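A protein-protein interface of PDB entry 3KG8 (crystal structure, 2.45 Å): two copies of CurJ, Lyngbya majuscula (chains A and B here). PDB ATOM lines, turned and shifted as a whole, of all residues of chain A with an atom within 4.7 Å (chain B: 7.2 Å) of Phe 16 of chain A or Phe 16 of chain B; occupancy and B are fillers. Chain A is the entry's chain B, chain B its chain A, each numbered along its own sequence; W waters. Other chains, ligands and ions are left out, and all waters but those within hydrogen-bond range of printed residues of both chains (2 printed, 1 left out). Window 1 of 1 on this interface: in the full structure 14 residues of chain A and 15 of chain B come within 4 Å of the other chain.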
ATOM      1  N   GLN A  14       3.433 -21.202 -19.813  1.00  0.00           N
ATOM      2  CA  GLN A  14       2.134 -20.848 -20.366  1.00  0.00           C
ATOM      3  C   GLN A  14       1.137 -20.286 -19.352  1.00  0.00           C
ATOM      4  O   GLN A  14       1.180 -20.599 -18.165  1.00  0.00           O
ATOM      5  CB  GLN A  14       1.543 -21.998 -21.228  1.00  0.00           C
ATOM      6  CG  GLN A  14       0.503 -22.936 -20.569  1.00  0.00           C
ATOM      7  CD  GLN A  14      -0.357 -23.722 -21.596  1.00  0.00           C
ATOM      8  OE1 GLN A  14      -1.028 -23.133 -22.455  1.00  0.00           O
ATOM      9  NE2 GLN A  14      -0.342 -25.055 -21.491  1.00  0.00           N
ATOM     10  N   LYS A  15       0.280 -19.406 -19.861  1.00  0.00           N
ATOM     11  CA  LYS A  15      -0.906 -18.931 -19.186  1.00  0.00           C
ATOM     12  C   LYS A  15      -2.104 -19.514 -19.935  1.00  0.00           C
ATOM     13  O   LYS A  15      -2.110 -19.551 -21.164  1.00  0.00           O
ATOM     14  CB  LYS A  15      -0.965 -17.401 -19.229  1.00  0.00           C
ATOM     15  CG  LYS A  15      -2.237 -16.814 -18.627  1.00  0.00           C
ATOM     16  CD  LYS A  15      -2.247 -15.299 -18.688  1.00  0.00           C
ATOM     17  CE  LYS A  15      -3.616 -14.766 -18.283  1.00  0.00           C
ATOM     18  NZ  LYS A  15      -3.546 -13.573 -17.395  1.00  0.00           N
ATOM     19  N   PHE A  16      -3.112 -19.975 -19.203  1.00  0.00           N
ATOM     20  CA  PHE A  16      -4.335 -20.407 -19.842  1.00  0.00           C
ATOM     21  C   PHE A  16      -5.607 -19.893 -19.184  1.00  0.00           C
ATOM     22  O   PHE A  16      -5.799 -20.026 -17.984  1.00  0.00           O
ATOM     23  CB  PHE A  16      -4.405 -21.927 -19.961  1.00  0.00           C
ATOM     24  CG  PHE A  16      -5.606 -22.376 -20.708  1.00  0.00           C
ATOM     25  CD1 PHE A  16      -5.636 -22.292 -22.095  1.00  0.00           C
ATOM     26  CD2 PHE A  16      -6.745 -22.797 -20.031  1.00  0.00           C
ATOM     27  CE1 PHE A  16      -6.768 -22.660 -22.815  1.00  0.00           C
ATOM     28  CE2 PHE A  16      -7.880 -23.168 -20.743  1.00  0.00           C
ATOM     29  CZ  PHE A  16      -7.881 -23.093 -22.139  1.00  0.00           C
ATOM     30  N   GLN A  17      -6.478 -19.294 -19.982  1.00  0.00           N
ATOM     31  CA  GLN A  17      -7.818 -18.974 -19.508  1.00  0.00           C
ATOM     32  C   GLN A  17      -8.843 -19.200 -20.588  1.00  0.00           C
ATOM     33  O   GLN A  17      -8.516 -19.214 -21.788  1.00  0.00           O
ATOM     34  CB  GLN A  17      -7.921 -17.551 -18.953  1.00  0.00           C
ATOM     35  CG  GLN A  17      -7.831 -16.452 -19.975  1.00  0.00           C
ATOM     36  CD  GLN A  17      -7.093 -15.238 -19.442  1.00  0.00           C
ATOM     37  OE1 GLN A  17      -7.093 -14.974 -18.238  1.00  0.00           O
ATOM     38  NE2 GLN A  17      -6.441 -14.498 -20.343  1.00  0.00           N
ATOM     39  N   SER A  18     -10.080 -19.387 -20.143  1.00  0.00           N
ATOM     40  CA  SER A  18     -11.185 -19.589 -21.042  1.00  0.00           C
ATOM     41  C   SER A  18     -12.448 -18.932 -20.485  1.00  0.00           C
ATOM     42  O   SER A  18     -12.623 -18.848 -19.275  1.00  0.00           O
ATOM     43  CB  SER A  18     -11.405 -21.089 -21.249  1.00  0.00           C
ATOM     44  OG  SER A  18     -12.493 -21.323 -22.129  1.00  0.00           O
ATOM     45  N   GLU A  23     -11.436 -20.680 -13.291  1.00  0.00           N
ATOM     46  CA  GLU A  23     -10.034 -20.620 -12.896  1.00  0.00           C
ATOM     47  C   GLU A  23      -9.106 -20.076 -13.969  1.00  0.00           C
ATOM     48  O   GLU A  23      -9.341 -20.268 -15.162  1.00  0.00           O
ATOM     49  CB  GLU A  23      -9.560 -22.017 -12.498  1.00  0.00           C
ATOM     50  CG  GLU A  23     -10.465 -22.727 -11.491  1.00  0.00           C
ATOM     51  CD  GLU A  23     -11.590 -23.522 -12.141  1.00  0.00           C
ATOM     52  OE1 GLU A  23     -12.183 -24.364 -11.443  1.00  0.00           O
ATOM     53  OE2 GLU A  23     -11.892 -23.323 -13.339  1.00  0.00           O
ATOM     54  N   ILE A  24      -8.043 -19.414 -13.532  1.00  0.00           N
ATOM     55  CA  ILE A  24      -6.962 -18.969 -14.412  1.00  0.00           C
ATOM     56  C   ILE A  24      -5.737 -19.817 -14.100  1.00  0.00           C
ATOM     57  O   ILE A  24      -5.419 -20.041 -12.941  1.00  0.00           O
ATOM     58  CB  ILE A  24      -6.654 -17.463 -14.223  1.00  0.00           C
ATOM     59  CG1 ILE A  24      -7.881 -16.622 -14.621  1.00  0.00           C
ATOM     60  CG2 ILE A  24      -5.426 -17.049 -15.040  1.00  0.00           C
ATOM     61  CD1 ILE A  24      -7.863 -15.176 -14.130  1.00  0.00           C
ATOM     62  N   PHE A  25      -5.054 -20.295 -15.133  1.00  0.00           N
ATOM     63  CA  PHE A  25      -4.000 -21.283 -14.954  1.00  0.00           C
ATOM     64  C   PHE A  25      -2.663 -20.799 -15.485  1.00  0.00           C
ATOM     65  O   PHE A  25      -2.599 -20.127 -16.514  1.00  0.00           O
ATOM     66  CB  PHE A  25      -4.348 -22.568 -15.703  1.00  0.00           C
ATOM     67  CG  PHE A  25      -5.663 -23.200 -15.307  1.00  0.00           C
ATOM     68  CD1 PHE A  25      -5.700 -24.242 -14.389  1.00  0.00           C
ATOM     69  CD2 PHE A  25      -6.859 -22.787 -15.892  1.00  0.00           C
ATOM     70  CE1 PHE A  25      -6.910 -24.858 -14.055  1.00  0.00           C
ATOM     71  CE2 PHE A  25      -8.076 -23.398 -15.564  1.00  0.00           C
ATOM     72  CZ  PHE A  25      -8.100 -24.429 -14.648  1.00  0.00           C
ATOM     73  N   GLU A  27       1.402 -22.490 -16.191  1.00  0.00           N
ATOM     74  CA  GLU A  27       2.069 -23.767 -16.316  1.00  0.00           C
ATOM     75  C   GLU A  27       3.564 -23.577 -16.502  1.00  0.00           C
ATOM     76  O   GLU A  27       4.002 -22.829 -17.379  1.00  0.00           O
ATOM     77  CB  GLU A  27       1.470 -24.564 -17.478  1.00  0.00           C
ATOM     78  CG  GLU A  27       1.849 -26.033 -17.485  1.00  0.00           C
ATOM     79  CD  GLU A  27       0.915 -26.865 -18.339  1.00  0.00           C
ATOM     80  OE1 GLU A  27       1.147 -26.961 -19.567  1.00  0.00           O
ATOM     81  OE2 GLU A  27      -0.047 -27.436 -17.778  1.00  0.00           O
ATOM     82  N   GLN A  93       1.780 -26.162 -11.853  1.00  0.00           N
ATOM     83  CA  GLN A  93       0.654 -25.307 -12.202  1.00  0.00           C
ATOM     84  C   GLN A  93       0.195 -24.431 -11.043  1.00  0.00           C
ATOM     85  O   GLN A  93       0.054 -24.904  -9.910  1.00  0.00           O
ATOM     86  CB  GLN A  93      -0.529 -26.154 -12.690  1.00  0.00           C
ATOM     87  CG  GLN A  93      -0.365 -26.732 -14.089  1.00  0.00           C
ATOM     88  CD  GLN A  93      -1.524 -27.645 -14.487  1.00  0.00           C
ATOM     89  OE1 GLN A  93      -2.345 -28.023 -13.646  1.00  0.00           O
ATOM     90  NE2 GLN A  93      -1.590 -28.009 -15.773  1.00  0.00           N
ATOM     91  N   LEU B   8       1.783 -28.033 -31.733  1.00  0.00           N
ATOM     92  CA  LEU B   8       1.368 -29.425 -31.552  1.00  0.00           C
ATOM     93  C   LEU B   8       0.753 -30.014 -32.818  1.00  0.00           C
ATOM     94  O   LEU B   8       0.749 -31.225 -33.010  1.00  0.00           O
ATOM     95  CB  LEU B   8       0.334 -29.541 -30.419  1.00  0.00           C
ATOM     96  CG  LEU B   8       0.571 -28.868 -29.067  1.00  0.00           C
ATOM     97  CD1 LEU B   8      -0.630 -29.101 -28.183  1.00  0.00           C
ATOM     98  CD2 LEU B   8       1.858 -29.358 -28.378  1.00  0.00           C
ATOM     99  N   GLN B  14      -1.588 -24.843 -28.445  1.00  0.00           N
ATOM    100  CA  GLN B  14      -1.382 -25.540 -27.180  1.00  0.00           C
ATOM    101  C   GLN B  14      -2.568 -26.367 -26.724  1.00  0.00           C
ATOM    102  O   GLN B  14      -3.691 -26.181 -27.188  1.00  0.00           O
ATOM    103  CB  GLN B  14      -0.897 -24.604 -26.056  1.00  0.00           C
ATOM    104  CG  GLN B  14      -1.660 -23.297 -25.883  1.00  0.00           C
ATOM    105  CD  GLN B  14      -0.874 -22.082 -26.374  1.00  0.00           C
ATOM    106  OE1 GLN B  14      -1.346 -21.329 -27.238  1.00  0.00           O
ATOM    107  NE2 GLN B  14       0.337 -21.887 -25.822  1.00  0.00           N
ATOM    108  N   LYS B  15      -2.265 -27.302 -25.829  1.00  0.00           N
ATOM    109  CA  LYS B  15      -3.215 -28.135 -25.116  1.00  0.00           C
ATOM    110  C   LYS B  15      -3.113 -27.764 -23.638  1.00  0.00           C
ATOM    111  O   LYS B  15      -2.012 -27.599 -23.105  1.00  0.00           O
ATOM    112  CB  LYS B  15      -2.817 -29.600 -25.285  1.00  0.00           C
ATOM    113  CG  LYS B  15      -3.761 -30.609 -24.646  1.00  0.00           C
ATOM    114  CD  LYS B  15      -3.238 -32.037 -24.815  1.00  0.00           C
ATOM    115  CE  LYS B  15      -4.282 -33.051 -24.379  1.00  0.00           C
ATOM    116  NZ  LYS B  15      -3.701 -34.398 -24.171  1.00  0.00           N
ATOM    117  N   PHE B  16      -4.243 -27.635 -22.962  1.00  0.00           N
ATOM    118  CA  PHE B  16      -4.175 -27.464 -21.525  1.00  0.00           C
ATOM    119  C   PHE B  16      -5.058 -28.430 -20.763  1.00  0.00           C
ATOM    120  O   PHE B  16      -6.240 -28.582 -21.075  1.00  0.00           O
ATOM    121  CB  PHE B  16      -4.483 -26.033 -21.069  1.00  0.00           C
ATOM    122  CG  PHE B  16      -4.231 -25.844 -19.605  1.00  0.00           C
ATOM    123  CD1 PHE B  16      -2.942 -25.585 -19.143  1.00  0.00           C
ATOM    124  CD2 PHE B  16      -5.249 -26.034 -18.679  1.00  0.00           C
ATOM    125  CE1 PHE B  16      -2.684 -25.467 -17.787  1.00  0.00           C
ATOM    126  CE2 PHE B  16      -4.997 -25.924 -17.309  1.00  0.00           C
ATOM    127  CZ  PHE B  16      -3.717 -25.642 -16.869  1.00  0.00           C
ATOM    128  N   GLN B  17      -4.482 -29.062 -19.749  1.00  0.00           N
ATOM    129  CA  GLN B  17      -5.266 -29.855 -18.812  1.00  0.00           C
ATOM    130  C   GLN B  17      -4.652 -29.858 -17.433  1.00  0.00           C
ATOM    131  O   GLN B  17      -3.456 -29.644 -17.267  1.00  0.00           O
ATOM    132  CB  GLN B  17      -5.436 -31.287 -19.300  1.00  0.00           C
ATOM    133  CG  GLN B  17      -4.204 -32.145 -19.223  1.00  0.00           C
ATOM    134  CD  GLN B  17      -4.438 -33.489 -19.875  1.00  0.00           C
ATOM    135  OE1 GLN B  17      -5.403 -34.200 -19.552  1.00  0.00           O
ATOM    136  NE2 GLN B  17      -3.568 -33.840 -20.819  1.00  0.00           N
ATOM    137  N   SER B  18      -5.494 -30.121 -16.447  1.00  0.00           N
ATOM    138  CA  SER B  18      -5.110 -30.049 -15.053  1.00  0.00           C
ATOM    139  C   SER B  18      -5.953 -31.022 -14.254  1.00  0.00           C
ATOM    140  O   SER B  18      -7.135 -31.165 -14.516  1.00  0.00           O
ATOM    141  CB  SER B  18      -5.338 -28.634 -14.523  1.00  0.00           C
ATOM    142  OG  SER B  18      -5.129 -28.588 -13.125  1.00  0.00           O
ATOM    143  N   PRO B  19      -5.337 -31.703 -13.278  1.00  0.00           N
ATOM    144  CA  PRO B  19      -6.039 -32.471 -12.247  1.00  0.00           C
ATOM    145  C   PRO B  19      -7.181 -31.688 -11.595  1.00  0.00           C
ATOM    146  O   PRO B  19      -8.091 -32.287 -11.018  1.00  0.00           O
ATOM    147  CB  PRO B  19      -4.950 -32.702 -11.203  1.00  0.00           C
ATOM    148  CG  PRO B  19      -3.686 -32.734 -11.986  1.00  0.00           C
ATOM    149  CD  PRO B  19      -3.871 -31.802 -13.146  1.00  0.00           C
ATOM    150  N   SER B  21      -9.072 -29.446 -13.275  1.00  0.00           N
ATOM    151  CA  SER B  21     -10.030 -29.053 -14.298  1.00  0.00           C
ATOM    152  C   SER B  21     -10.688 -30.300 -14.871  1.00  0.00           C
ATOM    153  O   SER B  21     -10.005 -31.280 -15.189  1.00  0.00           O
ATOM    154  CB  SER B  21      -9.340 -28.248 -15.403  1.00  0.00           C
ATOM    155  OG  SER B  21     -10.258 -27.868 -16.421  1.00  0.00           O
ATOM    156  N   GLU B  23     -12.467 -30.359 -17.727  1.00  0.00           N
ATOM    157  CA  GLU B  23     -12.340 -30.320 -19.177  1.00  0.00           C
ATOM    158  C   GLU B  23     -10.938 -30.145 -19.716  1.00  0.00           C
ATOM    159  O   GLU B  23     -10.025 -29.680 -19.034  1.00  0.00           O
ATOM    160  CB  GLU B  23     -13.290 -29.297 -19.835  1.00  0.00           C
ATOM    161  CG  GLU B  23     -13.536 -28.014 -19.098  1.00  0.00           C
ATOM    162  CD  GLU B  23     -14.620 -28.159 -18.054  1.00  0.00           C
ATOM    163  OE1 GLU B  23     -15.680 -28.746 -18.374  1.00  0.00           O
ATOM    164  OE2 GLU B  23     -14.403 -27.687 -16.917  1.00  0.00           O
ATOM    165  N   ILE B  24     -10.788 -30.535 -20.970  1.00  0.00           N
ATOM    166  CA  ILE B  24      -9.515 -30.466 -21.640  1.00  0.00           C
ATOM    167  C   ILE B  24      -9.637 -29.383 -22.688  1.00  0.00           C
ATOM    168  O   ILE B  24     -10.608 -29.354 -23.422  1.00  0.00           O
ATOM    169  CB  ILE B  24      -9.181 -31.815 -22.279  1.00  0.00           C
ATOM    170  CG1 ILE B  24      -9.056 -32.874 -21.186  1.00  0.00           C
ATOM    171  CG2 ILE B  24      -7.919 -31.724 -23.125  1.00  0.00           C
ATOM    172  CD1 ILE B  24      -9.194 -34.274 -21.717  1.00  0.00           C
ATOM    173  N   PHE B  25      -8.648 -28.496 -22.740  1.00  0.00           N
ATOM    174  CA  PHE B  25      -8.640 -27.391 -23.682  1.00  0.00           C
ATOM    175  C   PHE B  25      -7.535 -27.494 -24.736  1.00  0.00           C
ATOM    176  O   PHE B  25      -6.410 -27.918 -24.458  1.00  0.00           O
ATOM    177  CB  PHE B  25      -8.457 -26.085 -22.934  1.00  0.00           C
ATOM    178  CG  PHE B  25      -9.461 -25.852 -21.841  1.00  0.00           C
ATOM    179  CD1 PHE B  25     -10.562 -25.041 -22.057  1.00  0.00           C
ATOM    180  CD2 PHE B  25      -9.284 -26.404 -20.589  1.00  0.00           C
ATOM    181  CE1 PHE B  25     -11.490 -24.796 -21.042  1.00  0.00           C
ATOM    182  CE2 PHE B  25     -10.206 -26.167 -19.566  1.00  0.00           C
ATOM    183  CZ  PHE B  25     -11.315 -25.358 -19.803  1.00  0.00           C
ATOM    184  N   PHE B  26      -7.869 -27.069 -25.944  1.00  0.00           N
ATOM    185  CA  PHE B  26      -6.890 -26.811 -26.975  1.00  0.00           C
ATOM    186  C   PHE B  26      -7.046 -25.357 -27.397  1.00  0.00           C
ATOM    187  O   PHE B  26      -8.160 -24.832 -27.413  1.00  0.00           O
ATOM    188  CB  PHE B  26      -7.085 -27.764 -28.154  1.00  0.00           C
ATOM    189  CG  PHE B  26      -6.923 -29.216 -27.788  1.00  0.00           C
ATOM    190  CD1 PHE B  26      -5.697 -29.843 -27.919  1.00  0.00           C
ATOM    191  CD2 PHE B  26      -7.994 -29.948 -27.289  1.00  0.00           C
ATOM    192  CE1 PHE B  26      -5.541 -31.182 -27.576  1.00  0.00           C
ATOM    193  CE2 PHE B  26      -7.849 -31.281 -26.938  1.00  0.00           C
ATOM    194  CZ  PHE B  26      -6.626 -31.899 -27.087  1.00  0.00           C
ATOM    195  N   GLU B  27      -5.925 -24.698 -27.688  1.00  0.00           N
ATOM    196  CA  GLU B  27      -5.937 -23.301 -28.094  1.00  0.00           C
ATOM    197  C   GLU B  27      -5.202 -23.140 -29.397  1.00  0.00           C
ATOM    198  O   GLU B  27      -4.217 -23.834 -29.689  1.00  0.00           O
ATOM    199  CB  GLU B  27      -5.309 -22.396 -27.031  1.00  0.00           C
ATOM    200  CG  GLU B  27      -5.660 -20.924 -27.171  1.00  0.00           C
ATOM    201  CD  GLU B  27      -5.239 -20.098 -25.960  1.00  0.00           C
ATOM    202  OE1 GLU B  27      -6.095 -19.840 -25.089  1.00  0.00           O
ATOM    203  OE2 GLU B  27      -4.052 -19.711 -25.868  1.00  0.00           O
ATOM    204  N   THR B  91      -8.713 -15.897 -31.056  1.00  0.00           N
ATOM    205  CA  THR B  91      -8.344 -17.090 -30.335  1.00  0.00           C
ATOM    206  C   THR B  91      -9.493 -18.089 -30.447  1.00  0.00           C
ATOM    207  O   THR B  91     -10.646 -17.735 -30.212  1.00  0.00           O
ATOM    208  CB  THR B  91      -8.046 -16.754 -28.854  1.00  0.00           C
ATOM    209  OG1 THR B  91      -6.916 -15.867 -28.784  1.00  0.00           O
ATOM    210  CG2 THR B  91      -7.756 -17.997 -28.065  1.00  0.00           C
ATOM    211  N   GLN B  93     -10.729 -21.927 -29.117  1.00  0.00           N
ATOM    212  CA  GLN B  93     -10.503 -23.048 -28.211  1.00  0.00           C
ATOM    213  C   GLN B  93     -11.458 -24.195 -28.483  1.00  0.00           C
ATOM    214  O   GLN B  93     -12.641 -23.971 -28.762  1.00  0.00           O
ATOM    215  CB  GLN B  93     -10.641 -22.619 -26.756  1.00  0.00           C
ATOM    216  CG  GLN B  93      -9.663 -21.549 -26.382  1.00  0.00           C
ATOM    217  CD  GLN B  93      -9.855 -21.031 -24.990  1.00  0.00           C
ATOM    218  OE1 GLN B  93     -10.941 -21.113 -24.433  1.00  0.00           O
ATOM    219  NE2 GLN B  93      -8.797 -20.480 -24.421  1.00  0.00           N
ATOM    220  N   VAL B  94     -10.923 -25.412 -28.426  1.00  0.00           N
ATOM    221  CA  VAL B  94     -11.739 -26.608 -28.314  1.00  0.00           C
ATOM    222  C   VAL B  94     -11.814 -26.951 -26.838  1.00  0.00           C
ATOM    223  O   VAL B  94     -10.793 -27.053 -26.153  1.00  0.00           O
ATOM    224  CB  VAL B  94     -11.163 -27.777 -29.103  1.00  0.00           C
ATOM    225  CG1 VAL B  94     -12.155 -28.974 -29.103  1.00  0.00           C
ATOM    226  CG2 VAL B  94     -10.854 -27.334 -30.528  1.00  0.00           C
ATOM    227  N   VAL B  95     -13.037 -27.080 -26.338  1.00  0.00           N
ATOM    228  CA  VAL B  95     -13.254 -27.381 -24.944  1.00  0.00           C
ATOM    229  C   VAL B  95     -13.925 -28.746 -24.880  1.00  0.00           C
ATOM    230  O   VAL B  95     -15.060 -28.899 -25.322  1.00  0.00           O
ATOM    231  CB  VAL B  95     -14.146 -26.327 -24.271  1.00  0.00           C
ATOM    232  CG1 VAL B  95     -14.312 -26.650 -22.783  1.00  0.00           C
ATOM    233  CG2 VAL B  95     -13.563 -24.930 -24.462  1.00  0.00           C
ATOM    234  N   PHE B 110     -12.879 -15.975 -29.371  1.00  0.00           N
ATOM    235  CA  PHE B 110     -12.940 -14.627 -28.819  1.00  0.00           C
ATOM    236  C   PHE B 110     -11.737 -13.787 -29.266  1.00  0.00           C
ATOM    237  O   PHE B 110     -10.647 -14.325 -29.521  1.00  0.00           O
ATOM    238  CB  PHE B 110     -13.021 -14.665 -27.281  1.00  0.00           C
ATOM    239  CG  PHE B 110     -11.926 -15.449 -26.639  1.00  0.00           C
ATOM    240  CD1 PHE B 110     -12.046 -16.827 -26.479  1.00  0.00           C
ATOM    241  CD2 PHE B 110     -10.761 -14.811 -26.201  1.00  0.00           C
ATOM    242  CE1 PHE B 110     -11.025 -17.570 -25.889  1.00  0.00           C
ATOM    243  CE2 PHE B 110      -9.725 -15.532 -25.607  1.00  0.00           C
ATOM    244  CZ  PHE B 110      -9.857 -16.911 -25.440  1.00  0.00           C
HETATM  245  O   HOH W   1      -5.429 -18.614 -22.965  1.00  0.00           O
HETATM  246  O   HOH W   2      -1.387 -28.403 -19.899  1.00  0.00           O
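Among the printed residues, pairs that only touch across the chains: Phe 16 of chain A with Phe 25 of chain B, Glu 27 of chain A with Phe 16 of chain B, Phe 25 of chain A with Phe 16 of chain B, Gln 93 of chain A with Phe 16 of chain B, Phe 16 of chain A with Gln 93 of chain B, Gln 14 of chain A with Gln 14 of chain B, Gln 14 of chain A with Phe 16 of chain B, Phe 16 of chain A with Glu 27 of chain B, Ser 18 of chain A with Phe 25 of chain B and Phe 16 of chain A with Phe 16 of chain B.
Of chain B, only Phe 16, Phe 25, Glu 27 and Gln 93 come within 4 Å of Phe 16 of chain A. Of the printed residues of chain B, Gln 17 of chain A touches Gln 93. Of the printed residues of chain B, Ser 18 of chain A touches Phe 25 (3.7 Å) and Gln 93 (2.8 Å). Phe 16 of chain B touches just these residues of chain A: Gln 14 (3.5 Å), Phe 16 (3.8 Å), Phe 25 (3.3 Å), Glu 27 (3.3 Å) and Gln 93 (3.4 Å). The nearest residue of chain B that does not touch Phe 16 of chain A is Phe 26 of chain B (5.3 Å). The nearest printed residue of chain A that does not touch Phe 16 of chain B is Lys 15 of chain A (6.2 Å).
OE2 of Glu 27 of chain A sits at hydrogen-bond distance from NE2 of Gln 93 of chain A, 2.6 Å away. The backbone carbonyl oxygen (O) of Phe 25 of chain A sits at hydrogen-bond distance from the backbone NH (N) of Phe 16 of chain A, at 2.7 Å. The backbone NH (N) of Phe 16 of chain B is in hydrogen-bond range of the backbone carbonyl oxygen (O) of Phe 25 of chain B (2.6 Å). O of Gln 14 of chain A lies within hydrogen-bond range of N of Glu 27 of chain A (2.7 Å). O of Gln 14 of chain B is in hydrogen-bond range of N of Glu 27 of chain B (2.7 Å). OE1 of Glu 27 of chain B is in hydrogen-bond range of NE2 of Gln 93 of chain B (2.9 Å).
Phe 16 of chain B touches its own counterpart, Phe 16 of chain A. Phe 16 of chain A touches Phe 25 of chain B, and with the chains exchanged Phe 25 of chain A touches Phe 16 of chain B. Phe 16 of chain A touches Gln 93 of chain B, and with the chains exchanged Gln 93 of chain A touches Phe 16 of chain B. Ser 18 of chain A touches Gln 93 of chain B, and with the chains exchanged Gln 93 of chain A touches Ser 18 of chain B. Positions printed for both chains: 14, 15, 16, 17, 18, 23, 24, 25, 27 and 93.
Water W1 lies within hydrogen-bond range of OE1 of Glu 27 of chain B and N of Gln 17 of chain A. Water W2 lies within hydrogen-bond range of OE2 of Glu 27 of chain A, N of Gln 17 of chain B and O of Lys 15 of chain B.
Of the 18 printed residues of chain B, 8 touch a printed residue of chain A. Hydrophobic or aromatic side chains of chain B that line the printed part of chain A: Phe 16 and Phe 25. Hydrophobic or aromatic side chains of chain A within 4 Å of the printed part of chain B: Phe 16 and Phe 25. Among the printed residues, 15 pairs touch across the chains. Among the printed residues, no Asp or Glu carboxylate lies within 4 Å of a Lys or Arg side-chain nitrogen of the other chain.
The side-chain amide oxygen of Gln 93 of chain A lies within hydrogen-bond range of the side-chain hydroxyl of Ser 18 of chain B, at 2.9 Å. OE1 of Gln 93 of chain B is in hydrogen-bond range of OG of Ser 18 of chain A, 2.8 Å away. O of Lys 15 of chain B lies within hydrogen-bond range of NE2 of Gln 14 of chain A (3.4 Å). NE2 of Gln 93 of chain B lies within hydrogen-bond range of O of Gln 17 of chain A. O of Gln 17 of chain B is in hydrogen-bond range of NE2 of Gln 93 of chain A, 2.9 Å away.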
